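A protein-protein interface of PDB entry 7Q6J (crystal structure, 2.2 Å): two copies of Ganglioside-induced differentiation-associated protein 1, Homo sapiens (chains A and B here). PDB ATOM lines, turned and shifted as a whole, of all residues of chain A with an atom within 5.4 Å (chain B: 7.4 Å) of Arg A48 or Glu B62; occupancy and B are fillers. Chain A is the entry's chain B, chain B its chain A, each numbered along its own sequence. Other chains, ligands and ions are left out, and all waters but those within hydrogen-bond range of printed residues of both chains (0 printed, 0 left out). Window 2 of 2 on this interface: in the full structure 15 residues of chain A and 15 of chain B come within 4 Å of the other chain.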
ATOM      1  N   TRP A   9     -22.668 -10.427  -0.356  1.00  0.00           N
ATOM      2  CA  TRP A   9     -21.953  -9.434  -1.175  1.00  0.00           C
ATOM      3  C   TRP A   9     -22.477  -9.495  -2.599  1.00  0.00           C
ATOM      4  O   TRP A   9     -22.403 -10.552  -3.228  1.00  0.00           O
ATOM      5  CB  TRP A   9     -20.446  -9.688  -1.288  1.00  0.00           C
ATOM      6  CG  TRP A   9     -19.757  -9.945  -0.024  1.00  0.00           C
ATOM      7  CD1 TRP A   9     -18.965  -9.064   0.680  1.00  0.00           C
ATOM      8  CD2 TRP A   9     -19.738 -11.194   0.697  1.00  0.00           C
ATOM      9  NE1 TRP A   9     -18.508  -9.689   1.833  1.00  0.00           N
ATOM     10  CE2 TRP A   9     -18.953 -10.997   1.852  1.00  0.00           C
ATOM     11  CE3 TRP A   9     -20.312 -12.460   0.477  1.00  0.00           C
ATOM     12  CZ2 TRP A   9     -18.742 -12.020   2.787  1.00  0.00           C
ATOM     13  CZ3 TRP A   9     -20.112 -13.458   1.406  1.00  0.00           C
ATOM     14  CH2 TRP A   9     -19.337 -13.238   2.540  1.00  0.00           C
ATOM     15  N   VAL A  34     -23.362  -6.151   2.209  1.00  0.00           N
ATOM     16  CA  VAL A  34     -22.425  -5.605   3.183  1.00  0.00           C
ATOM     17  C   VAL A  34     -21.088  -5.194   2.578  1.00  0.00           C
ATOM     18  O   VAL A  34     -20.217  -4.718   3.311  1.00  0.00           O
ATOM     19  CB  VAL A  34     -22.234  -6.631   4.322  1.00  0.00           C
ATOM     20  CG1 VAL A  34     -23.576  -7.084   4.864  1.00  0.00           C
ATOM     21  CG2 VAL A  34     -21.460  -7.855   3.872  1.00  0.00           C
ATOM     22  N   SER A  35     -20.910  -5.337   1.266  1.00  0.00           N
ATOM     23  CA  SER A  35     -19.663  -4.935   0.626  1.00  0.00           C
ATOM     24  C   SER A  35     -19.606  -3.422   0.505  1.00  0.00           C
ATOM     25  O   SER A  35     -20.626  -2.748   0.375  1.00  0.00           O
ATOM     26  CB  SER A  35     -19.548  -5.523  -0.772  1.00  0.00           C
ATOM     27  OG  SER A  35     -20.699  -5.168  -1.498  1.00  0.00           O
ATOM     28  N   LEU A  36     -18.474  -2.928   0.546  1.00  0.00           N
ATOM     29  CA  LEU A  36     -18.203  -1.499   0.448  1.00  0.00           C
ATOM     30  C   LEU A  36     -17.675  -1.126  -0.933  1.00  0.00           C
ATOM     31  O   LEU A  36     -17.001  -1.930  -1.591  1.00  0.00           O
ATOM     32  CB  LEU A  36     -17.195  -1.083   1.512  1.00  0.00           C
ATOM     33  CG  LEU A  36     -17.770  -1.120   2.945  1.00  0.00           C
ATOM     34  CD1 LEU A  36     -16.671  -0.760   3.953  1.00  0.00           C
ATOM     35  CD2 LEU A  36     -18.994  -0.200   3.062  1.00  0.00           C
ATOM     36  N   LEU A  38     -15.357   0.887  -1.857  1.00  0.00           N
ATOM     37  CA  LEU A  38     -13.908   0.850  -1.824  1.00  0.00           C
ATOM     38  C   LEU A  38     -13.463   0.237  -0.511  1.00  0.00           C
ATOM     39  O   LEU A  38     -14.043   0.525   0.547  1.00  0.00           O
ATOM     40  CB  LEU A  38     -13.314   2.247  -1.965  1.00  0.00           C
ATOM     41  CG  LEU A  38     -13.379   2.820  -3.389  1.00  0.00           C
ATOM     42  CD1 LEU A  38     -12.914   4.301  -3.365  1.00  0.00           C
ATOM     43  CD2 LEU A  38     -12.553   2.007  -4.370  1.00  0.00           C
ATOM     44  N   SER A  39     -12.455  -0.632  -0.614  1.00  0.00           N
ATOM     45  CA  SER A  39     -11.775  -1.236   0.516  1.00  0.00           C
ATOM     46  C   SER A  39     -10.831  -0.227   1.178  1.00  0.00           C
ATOM     47  O   SER A  39     -10.675   0.915   0.727  1.00  0.00           O
ATOM     48  CB  SER A  39     -10.979  -2.455   0.058  1.00  0.00           C
ATOM     49  OG  SER A  39      -9.765  -2.047  -0.563  1.00  0.00           O
ATOM     50  N   GLU A  43      -9.309  -0.202  -3.160  1.00  0.00           N
ATOM     51  CA  GLU A  43      -9.603  -1.166  -4.221  1.00  0.00           C
ATOM     52  C   GLU A  43     -11.114  -1.287  -4.450  1.00  0.00           C
ATOM     53  O   GLU A  43     -11.887  -1.373  -3.486  1.00  0.00           O
ATOM     54  CB  GLU A  43      -9.065  -2.545  -3.860  1.00  0.00           C
ATOM     55  CG  GLU A  43      -7.543  -2.680  -3.838  1.00  0.00           C
ATOM     56  CD  GLU A  43      -7.096  -4.005  -3.212  1.00  0.00           C
ATOM     57  OE1 GLU A  43      -7.744  -4.437  -2.227  1.00  0.00           O
ATOM     58  OE2 GLU A  43      -6.118  -4.616  -3.709  1.00  0.00           O
ATOM     59  N   PRO A  44     -11.579  -1.345  -5.708  1.00  0.00           N
ATOM     60  CA  PRO A  44     -13.022  -1.572  -5.938  1.00  0.00           C
ATOM     61  C   PRO A  44     -13.418  -3.030  -5.976  1.00  0.00           C
ATOM     62  O   PRO A  44     -12.565  -3.912  -5.874  1.00  0.00           O
ATOM     63  CB  PRO A  44     -13.273  -0.911  -7.307  1.00  0.00           C
ATOM     64  CG  PRO A  44     -11.939  -1.085  -8.030  1.00  0.00           C
ATOM     65  CD  PRO A  44     -10.867  -0.921  -6.937  1.00  0.00           C
ATOM     66  N   TRP A  45     -14.705  -3.306  -6.181  1.00  0.00           N
ATOM     67  CA  TRP A  45     -15.158  -4.677  -6.040  1.00  0.00           C
ATOM     68  C   TRP A  45     -14.409  -5.639  -6.946  1.00  0.00           C
ATOM     69  O   TRP A  45     -14.162  -6.791  -6.578  1.00  0.00           O
ATOM     70  CB  TRP A  45     -16.641  -4.761  -6.325  1.00  0.00           C
ATOM     71  CG  TRP A  45     -17.161  -4.444  -7.735  1.00  0.00           C
ATOM     72  CD1 TRP A  45     -17.666  -3.250  -8.163  1.00  0.00           C
ATOM     73  CD2 TRP A  45     -17.319  -5.360  -8.832  1.00  0.00           C
ATOM     74  NE1 TRP A  45     -18.134  -3.360  -9.457  1.00  0.00           N
ATOM     75  CE2 TRP A  45     -17.928  -4.644  -9.893  1.00  0.00           C
ATOM     76  CE3 TRP A  45     -16.999  -6.713  -9.025  1.00  0.00           C
ATOM     77  CZ2 TRP A  45     -18.232  -5.240 -11.145  1.00  0.00           C
ATOM     78  CZ3 TRP A  45     -17.341  -7.324 -10.264  1.00  0.00           C
ATOM     79  CH2 TRP A  45     -17.931  -6.574 -11.305  1.00  0.00           C
ATOM     80  N   PHE A  46     -14.068  -5.209  -8.151  1.00  0.00           N
ATOM     81  CA  PHE A  46     -13.555  -6.202  -9.089  1.00  0.00           C
ATOM     82  C   PHE A  46     -12.111  -6.602  -8.799  1.00  0.00           C
ATOM     83  O   PHE A  46     -11.669  -7.637  -9.319  1.00  0.00           O
ATOM     84  CB  PHE A  46     -13.688  -5.688 -10.545  1.00  0.00           C
ATOM     85  CG  PHE A  46     -13.038  -4.347 -10.778  1.00  0.00           C
ATOM     86  CD1 PHE A  46     -11.678  -4.262 -11.024  1.00  0.00           C
ATOM     87  CD2 PHE A  46     -13.796  -3.168 -10.792  1.00  0.00           C
ATOM     88  CE1 PHE A  46     -11.059  -3.009 -11.242  1.00  0.00           C
ATOM     89  CE2 PHE A  46     -13.192  -1.915 -11.009  1.00  0.00           C
ATOM     90  CZ  PHE A  46     -11.823  -1.829 -11.245  1.00  0.00           C
ATOM     91  N   MET A  47     -11.446  -5.929  -7.860  1.00  0.00           N
ATOM     92  CA  MET A  47     -10.113  -6.307  -7.411  1.00  0.00           C
ATOM     93  C   MET A  47     -10.149  -7.231  -6.205  1.00  0.00           C
ATOM     94  O   MET A  47      -9.091  -7.547  -5.659  1.00  0.00           O
ATOM     95  CB  MET A  47      -9.310  -5.069  -6.984  1.00  0.00           C
ATOM     96  CG  MET A  47      -9.015  -4.073  -8.059  1.00  0.00           C
ATOM     97  SD  MET A  47      -7.722  -4.645  -9.180  1.00  0.00           S
ATOM     98  CE  MET A  47      -6.309  -4.667  -8.068  1.00  0.00           C
ATOM     99  N   ARG A  48     -11.329  -7.662  -5.775  1.00  0.00           N
ATOM    100  CA  ARG A  48     -11.476  -8.316  -4.481  1.00  0.00           C
ATOM    101  C   ARG A  48     -12.326  -9.566  -4.584  1.00  0.00           C
ATOM    102  O   ARG A  48     -13.013  -9.925  -3.631  1.00  0.00           O
ATOM    103  CB  ARG A  48     -12.107  -7.362  -3.470  1.00  0.00           C
ATOM    104  CG  ARG A  48     -11.587  -5.925  -3.540  1.00  0.00           C
ATOM    105  CD  ARG A  48     -12.447  -4.997  -2.687  1.00  0.00           C
ATOM    106  NE  ARG A  48     -12.391  -5.441  -1.298  1.00  0.00           N
ATOM    107  CZ  ARG A  48     -13.238  -5.070  -0.345  1.00  0.00           C
ATOM    108  NH1 ARG A  48     -14.240  -4.240  -0.625  1.00  0.00           N
ATOM    109  NH2 ARG A  48     -13.079  -5.542   0.894  1.00  0.00           N
ATOM    110  N   LEU A  49     -12.305 -10.226  -5.733  1.00  0.00           N
ATOM    111  CA  LEU A  49     -13.133 -11.397  -5.933  1.00  0.00           C
ATOM    112  C   LEU A  49     -12.480 -12.640  -5.349  1.00  0.00           C
ATOM    113  O   LEU A  49     -11.248 -12.745  -5.250  1.00  0.00           O
ATOM    114  CB  LEU A  49     -13.424 -11.607  -7.419  1.00  0.00           C
ATOM    115  CG  LEU A  49     -14.138 -10.413  -8.080  1.00  0.00           C
ATOM    116  CD1 LEU A  49     -13.711 -10.194  -9.528  1.00  0.00           C
ATOM    117  CD2 LEU A  49     -15.654 -10.542  -7.935  1.00  0.00           C
ATOM    118  N   ASN A  50     -13.335 -13.577  -4.926  1.00  0.00           N
ATOM    119  CA  ASN A  50     -12.892 -14.874  -4.412  1.00  0.00           C
ATOM    120  C   ASN A  50     -11.832 -14.696  -3.326  1.00  0.00           C
ATOM    121  O   ASN A  50     -10.974 -15.559  -3.129  1.00  0.00           O
ATOM    122  CB  ASN A  50     -12.431 -15.784  -5.553  1.00  0.00           C
ATOM    123  CG  ASN A  50     -13.547 -16.014  -6.590  1.00  0.00           C
ATOM    124  OD1 ASN A  50     -13.671 -15.251  -7.553  1.00  0.00           O
ATOM    125  ND2 ASN A  50     -14.372 -17.051  -6.381  1.00  0.00           N
ATOM    126  N   SER A  51     -11.776 -13.489  -2.770  1.00  0.00           N
ATOM    127  CA  SER A  51     -11.098 -13.190  -1.524  1.00  0.00           C
ATOM    128  C   SER A  51     -11.965 -13.555  -0.318  1.00  0.00           C
ATOM    129  O   SER A  51     -13.198 -13.491  -0.372  1.00  0.00           O
ATOM    130  CB  SER A  51     -10.727 -11.709  -1.479  1.00  0.00           C
ATOM    131  OG  SER A  51     -11.761 -10.937  -0.895  1.00  0.00           O
ATOM    132  N   GLU A  54     -15.462 -16.440   2.849  1.00  0.00           N
ATOM    133  CA  GLU A  54     -16.699 -16.374   3.608  1.00  0.00           C
ATOM    134  C   GLU A  54     -17.885 -16.785   2.743  1.00  0.00           C
ATOM    135  O   GLU A  54     -17.784 -16.907   1.510  1.00  0.00           O
ATOM    136  CB  GLU A  54     -16.929 -14.964   4.141  1.00  0.00           C
ATOM    137  CG  GLU A  54     -15.881 -14.536   5.148  1.00  0.00           C
ATOM    138  CD  GLU A  54     -15.893 -13.038   5.432  1.00  0.00           C
ATOM    139  OE1 GLU A  54     -16.877 -12.326   5.094  1.00  0.00           O
ATOM    140  OE2 GLU A  54     -14.898 -12.574   6.007  1.00  0.00           O
ATOM    141  N   VAL B   2     -19.772   0.932  12.003  1.00  0.00           N
ATOM    142  CA  VAL B   2     -19.510  -0.501  11.886  1.00  0.00           C
ATOM    143  C   VAL B   2     -20.009  -1.248  13.123  1.00  0.00           C
ATOM    144  O   VAL B   2     -19.290  -1.464  14.107  1.00  0.00           O
ATOM    145  CB  VAL B   2     -18.022  -0.761  11.568  1.00  0.00           C
ATOM    146  CG1 VAL B   2     -17.112  -0.606  12.792  1.00  0.00           C
ATOM    147  CG2 VAL B   2     -17.882  -2.130  10.903  1.00  0.00           C
ATOM    148  N   ILE B  59     -21.945 -10.666  11.807  1.00  0.00           N
ATOM    149  CA  ILE B  59     -21.761  -9.714  10.733  1.00  0.00           C
ATOM    150  C   ILE B  59     -21.026  -8.521  11.301  1.00  0.00           C
ATOM    151  O   ILE B  59     -21.437  -7.960  12.325  1.00  0.00           O
ATOM    152  CB  ILE B  59     -23.114  -9.293  10.156  1.00  0.00           C
ATOM    153  CG1 ILE B  59     -23.864 -10.522   9.565  1.00  0.00           C
ATOM    154  CG2 ILE B  59     -22.921  -8.294   9.064  1.00  0.00           C
ATOM    155  CD1 ILE B  59     -25.042 -10.834  10.306  1.00  0.00           C
ATOM    156  N   HIS B  60     -19.961  -8.118  10.622  1.00  0.00           N
ATOM    157  CA  HIS B  60     -19.149  -7.017  11.094  1.00  0.00           C
ATOM    158  C   HIS B  60     -18.635  -6.291   9.861  1.00  0.00           C
ATOM    159  O   HIS B  60     -17.644  -6.716   9.263  1.00  0.00           O
ATOM    160  CB  HIS B  60     -18.015  -7.516  11.966  1.00  0.00           C
ATOM    161  CG  HIS B  60     -17.121  -6.426  12.437  1.00  0.00           C
ATOM    162  ND1 HIS B  60     -15.757  -6.477  12.287  1.00  0.00           N
ATOM    163  CD2 HIS B  60     -17.400  -5.241  13.027  1.00  0.00           C
ATOM    164  CE1 HIS B  60     -15.230  -5.361  12.767  1.00  0.00           C
ATOM    165  NE2 HIS B  60     -16.208  -4.591  13.212  1.00  0.00           N
ATOM    166  N   GLY B  61     -19.305  -5.206   9.505  1.00  0.00           N
ATOM    167  CA  GLY B  61     -18.983  -4.530   8.270  1.00  0.00           C
ATOM    168  C   GLY B  61     -19.154  -5.455   7.092  1.00  0.00           C
ATOM    169  O   GLY B  61     -20.206  -6.075   6.889  1.00  0.00           O
ATOM    170  N   GLU B  62     -18.078  -5.585   6.337  1.00  0.00           N
ATOM    171  CA  GLU B  62     -18.033  -6.407   5.146  1.00  0.00           C
ATOM    172  C   GLU B  62     -17.893  -7.892   5.454  1.00  0.00           C
ATOM    173  O   GLU B  62     -17.873  -8.707   4.528  1.00  0.00           O
ATOM    174  CB  GLU B  62     -16.833  -6.009   4.282  1.00  0.00           C
ATOM    175  CG  GLU B  62     -16.789  -4.612   3.808  1.00  0.00           C
ATOM    176  CD  GLU B  62     -15.789  -4.452   2.686  1.00  0.00           C
ATOM    177  OE1 GLU B  62     -14.584  -4.682   2.934  1.00  0.00           O
ATOM    178  OE2 GLU B  62     -16.226  -4.116   1.554  1.00  0.00           O
ATOM    179  N   ASN B  63     -17.681  -8.277   6.698  1.00  0.00           N
ATOM    180  CA  ASN B  63     -17.367  -9.669   7.030  1.00  0.00           C
ATOM    181  C   ASN B  63     -18.583 -10.431   7.569  1.00  0.00           C
ATOM    182  O   ASN B  63     -19.380  -9.898   8.346  1.00  0.00           O
ATOM    183  CB  ASN B  63     -16.232  -9.688   8.054  1.00  0.00           C
ATOM    184  CG  ASN B  63     -14.947  -9.166   7.479  1.00  0.00           C
ATOM    185  OD1 ASN B  63     -14.461  -8.090   7.856  1.00  0.00           O
ATOM    186  ND2 ASN B  63     -14.345  -9.956   6.605  1.00  0.00           N
ATOM    187  N   ILE B  64     -18.702 -11.682   7.157  1.00  0.00           N
ATOM    188  CA  ILE B  64     -19.753 -12.602   7.585  1.00  0.00           C
ATOM    189  C   ILE B  64     -19.033 -13.865   8.013  1.00  0.00           C
ATOM    190  O   ILE B  64     -18.231 -14.406   7.256  1.00  0.00           O
ATOM    191  CB  ILE B  64     -20.750 -12.901   6.456  1.00  0.00           C
ATOM    192  CG1 ILE B  64     -21.430 -11.603   5.999  1.00  0.00           C
ATOM    193  CG2 ILE B  64     -21.819 -13.871   6.919  1.00  0.00           C
ATOM    194  CD1 ILE B  64     -22.367 -11.738   4.739  1.00  0.00           C
ATOM    195  N   ILE B  65     -19.190 -14.241   9.260  1.00  0.00           N
ATOM    196  CA  ILE B  65     -18.477 -15.379   9.810  1.00  0.00           C
ATOM    197  C   ILE B  65     -19.489 -16.242  10.538  1.00  0.00           C
ATOM    198  O   ILE B  65     -20.209 -15.740  11.417  1.00  0.00           O
ATOM    199  CB  ILE B  65     -17.368 -14.933  10.797  1.00  0.00           C
ATOM    200  CG1 ILE B  65     -16.461 -13.888  10.157  1.00  0.00           C
ATOM    201  CG2 ILE B  65     -16.505 -16.093  11.193  1.00  0.00           C
ATOM    202  CD1 ILE B  65     -16.947 -12.516  10.403  1.00  0.00           C
ATOM    203  N   TYR B  74     -12.160 -14.635  14.908  1.00  0.00           N
ATOM    204  CA  TYR B  74     -12.273 -13.324  14.261  1.00  0.00           C
ATOM    205  C   TYR B  74     -12.274 -12.201  15.299  1.00  0.00           C
ATOM    206  O   TYR B  74     -11.596 -11.183  15.136  1.00  0.00           O
ATOM    207  CB  TYR B  74     -13.564 -13.270  13.392  1.00  0.00           C
ATOM    208  CG  TYR B  74     -13.806 -11.905  12.749  1.00  0.00           C
ATOM    209  CD1 TYR B  74     -13.200 -11.550  11.524  1.00  0.00           C
ATOM    210  CD2 TYR B  74     -14.622 -10.969  13.365  1.00  0.00           C
ATOM    211  CE1 TYR B  74     -13.378 -10.295  10.974  1.00  0.00           C
ATOM    212  CE2 TYR B  74     -14.806  -9.723  12.825  1.00  0.00           C
ATOM    213  CZ  TYR B  74     -14.218  -9.402  11.616  1.00  0.00           C
ATOM    214  OH  TYR B  74     -14.427  -8.133  11.096  1.00  0.00           O
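O of Glu B62 lies within hydrogen-bond range of NE1 of Trp A9, 2.9 Å away.
N of Leu A36 is in hydrogen-bond range of OE2 of Glu B62, 2.7 Å away.
OE1 of Glu B62 is in salt-bridge range of NH2 of Arg A48 (2.7 Å).
The side-chain amide nitrogen (ND2) of Asn B63 sits at hydrogen-bond distance from the side-chain carboxylate (OE2) of Glu A54 (2.7 Å).
The backbone NH (N) of Ile B64 is in hydrogen-bond range of the side-chain carboxylate (OE1) of Glu A54, 2.8 Å away.
The side-chain hydroxyl (OH) of Tyr B74 lies within hydrogen-bond range of the side-chain amide oxygen (OD1) of Asn B63, 3.2 Å away.
The backbone carbonyl oxygen (O) of Arg A48 is in hydrogen-bond range of the side-chain hydroxyl (OG) of Ser A51 (3.2 Å).
Gly B61 touches Val A34 (O to CB, 3.3 Å).
CA of Glu B62 touches O of Val A34, 3.3 Å away.
Glu B62 touches Ser A35 (OE2 to C, 3.6 Å).
O of Glu B62 touches OE1 of Glu A54, at 3.8 Å.
Of the printed residues of chain B, Trp A9 touches Glu B62 (2.9 Å).
Of the printed residues of chain B, Val A34 touches Gly B61 (3.3 Å) and Glu B62 (3.3 Å).
Of the printed residues of chain B, Ser A35 touches Glu B62 (3.6 Å).
Of the printed residues of chain B, Leu A36 touches Glu B62 (2.7 Å).
Arg A48 touches just one residue of chain B: Glu B62 (2.7 Å).
Of chain A, only Trp A9, Val A34, Ser A35, Leu A36, Arg A48 and Glu A54 come within 4 Å of Glu B62.
The nearest printed residue of chain B that does not touch Ser A35 is Gly B61 (5.7 Å).
Of the 16 printed residues of chain A, 6 touch a printed residue of chain B.
Of the 9 printed residues of chain B, 4 touch a printed residue of chain A.
No position is printed for both chains.
Of the 9 pairs that touch across the chains among the printed residues, none has its exchanged pair printed and touching as well.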
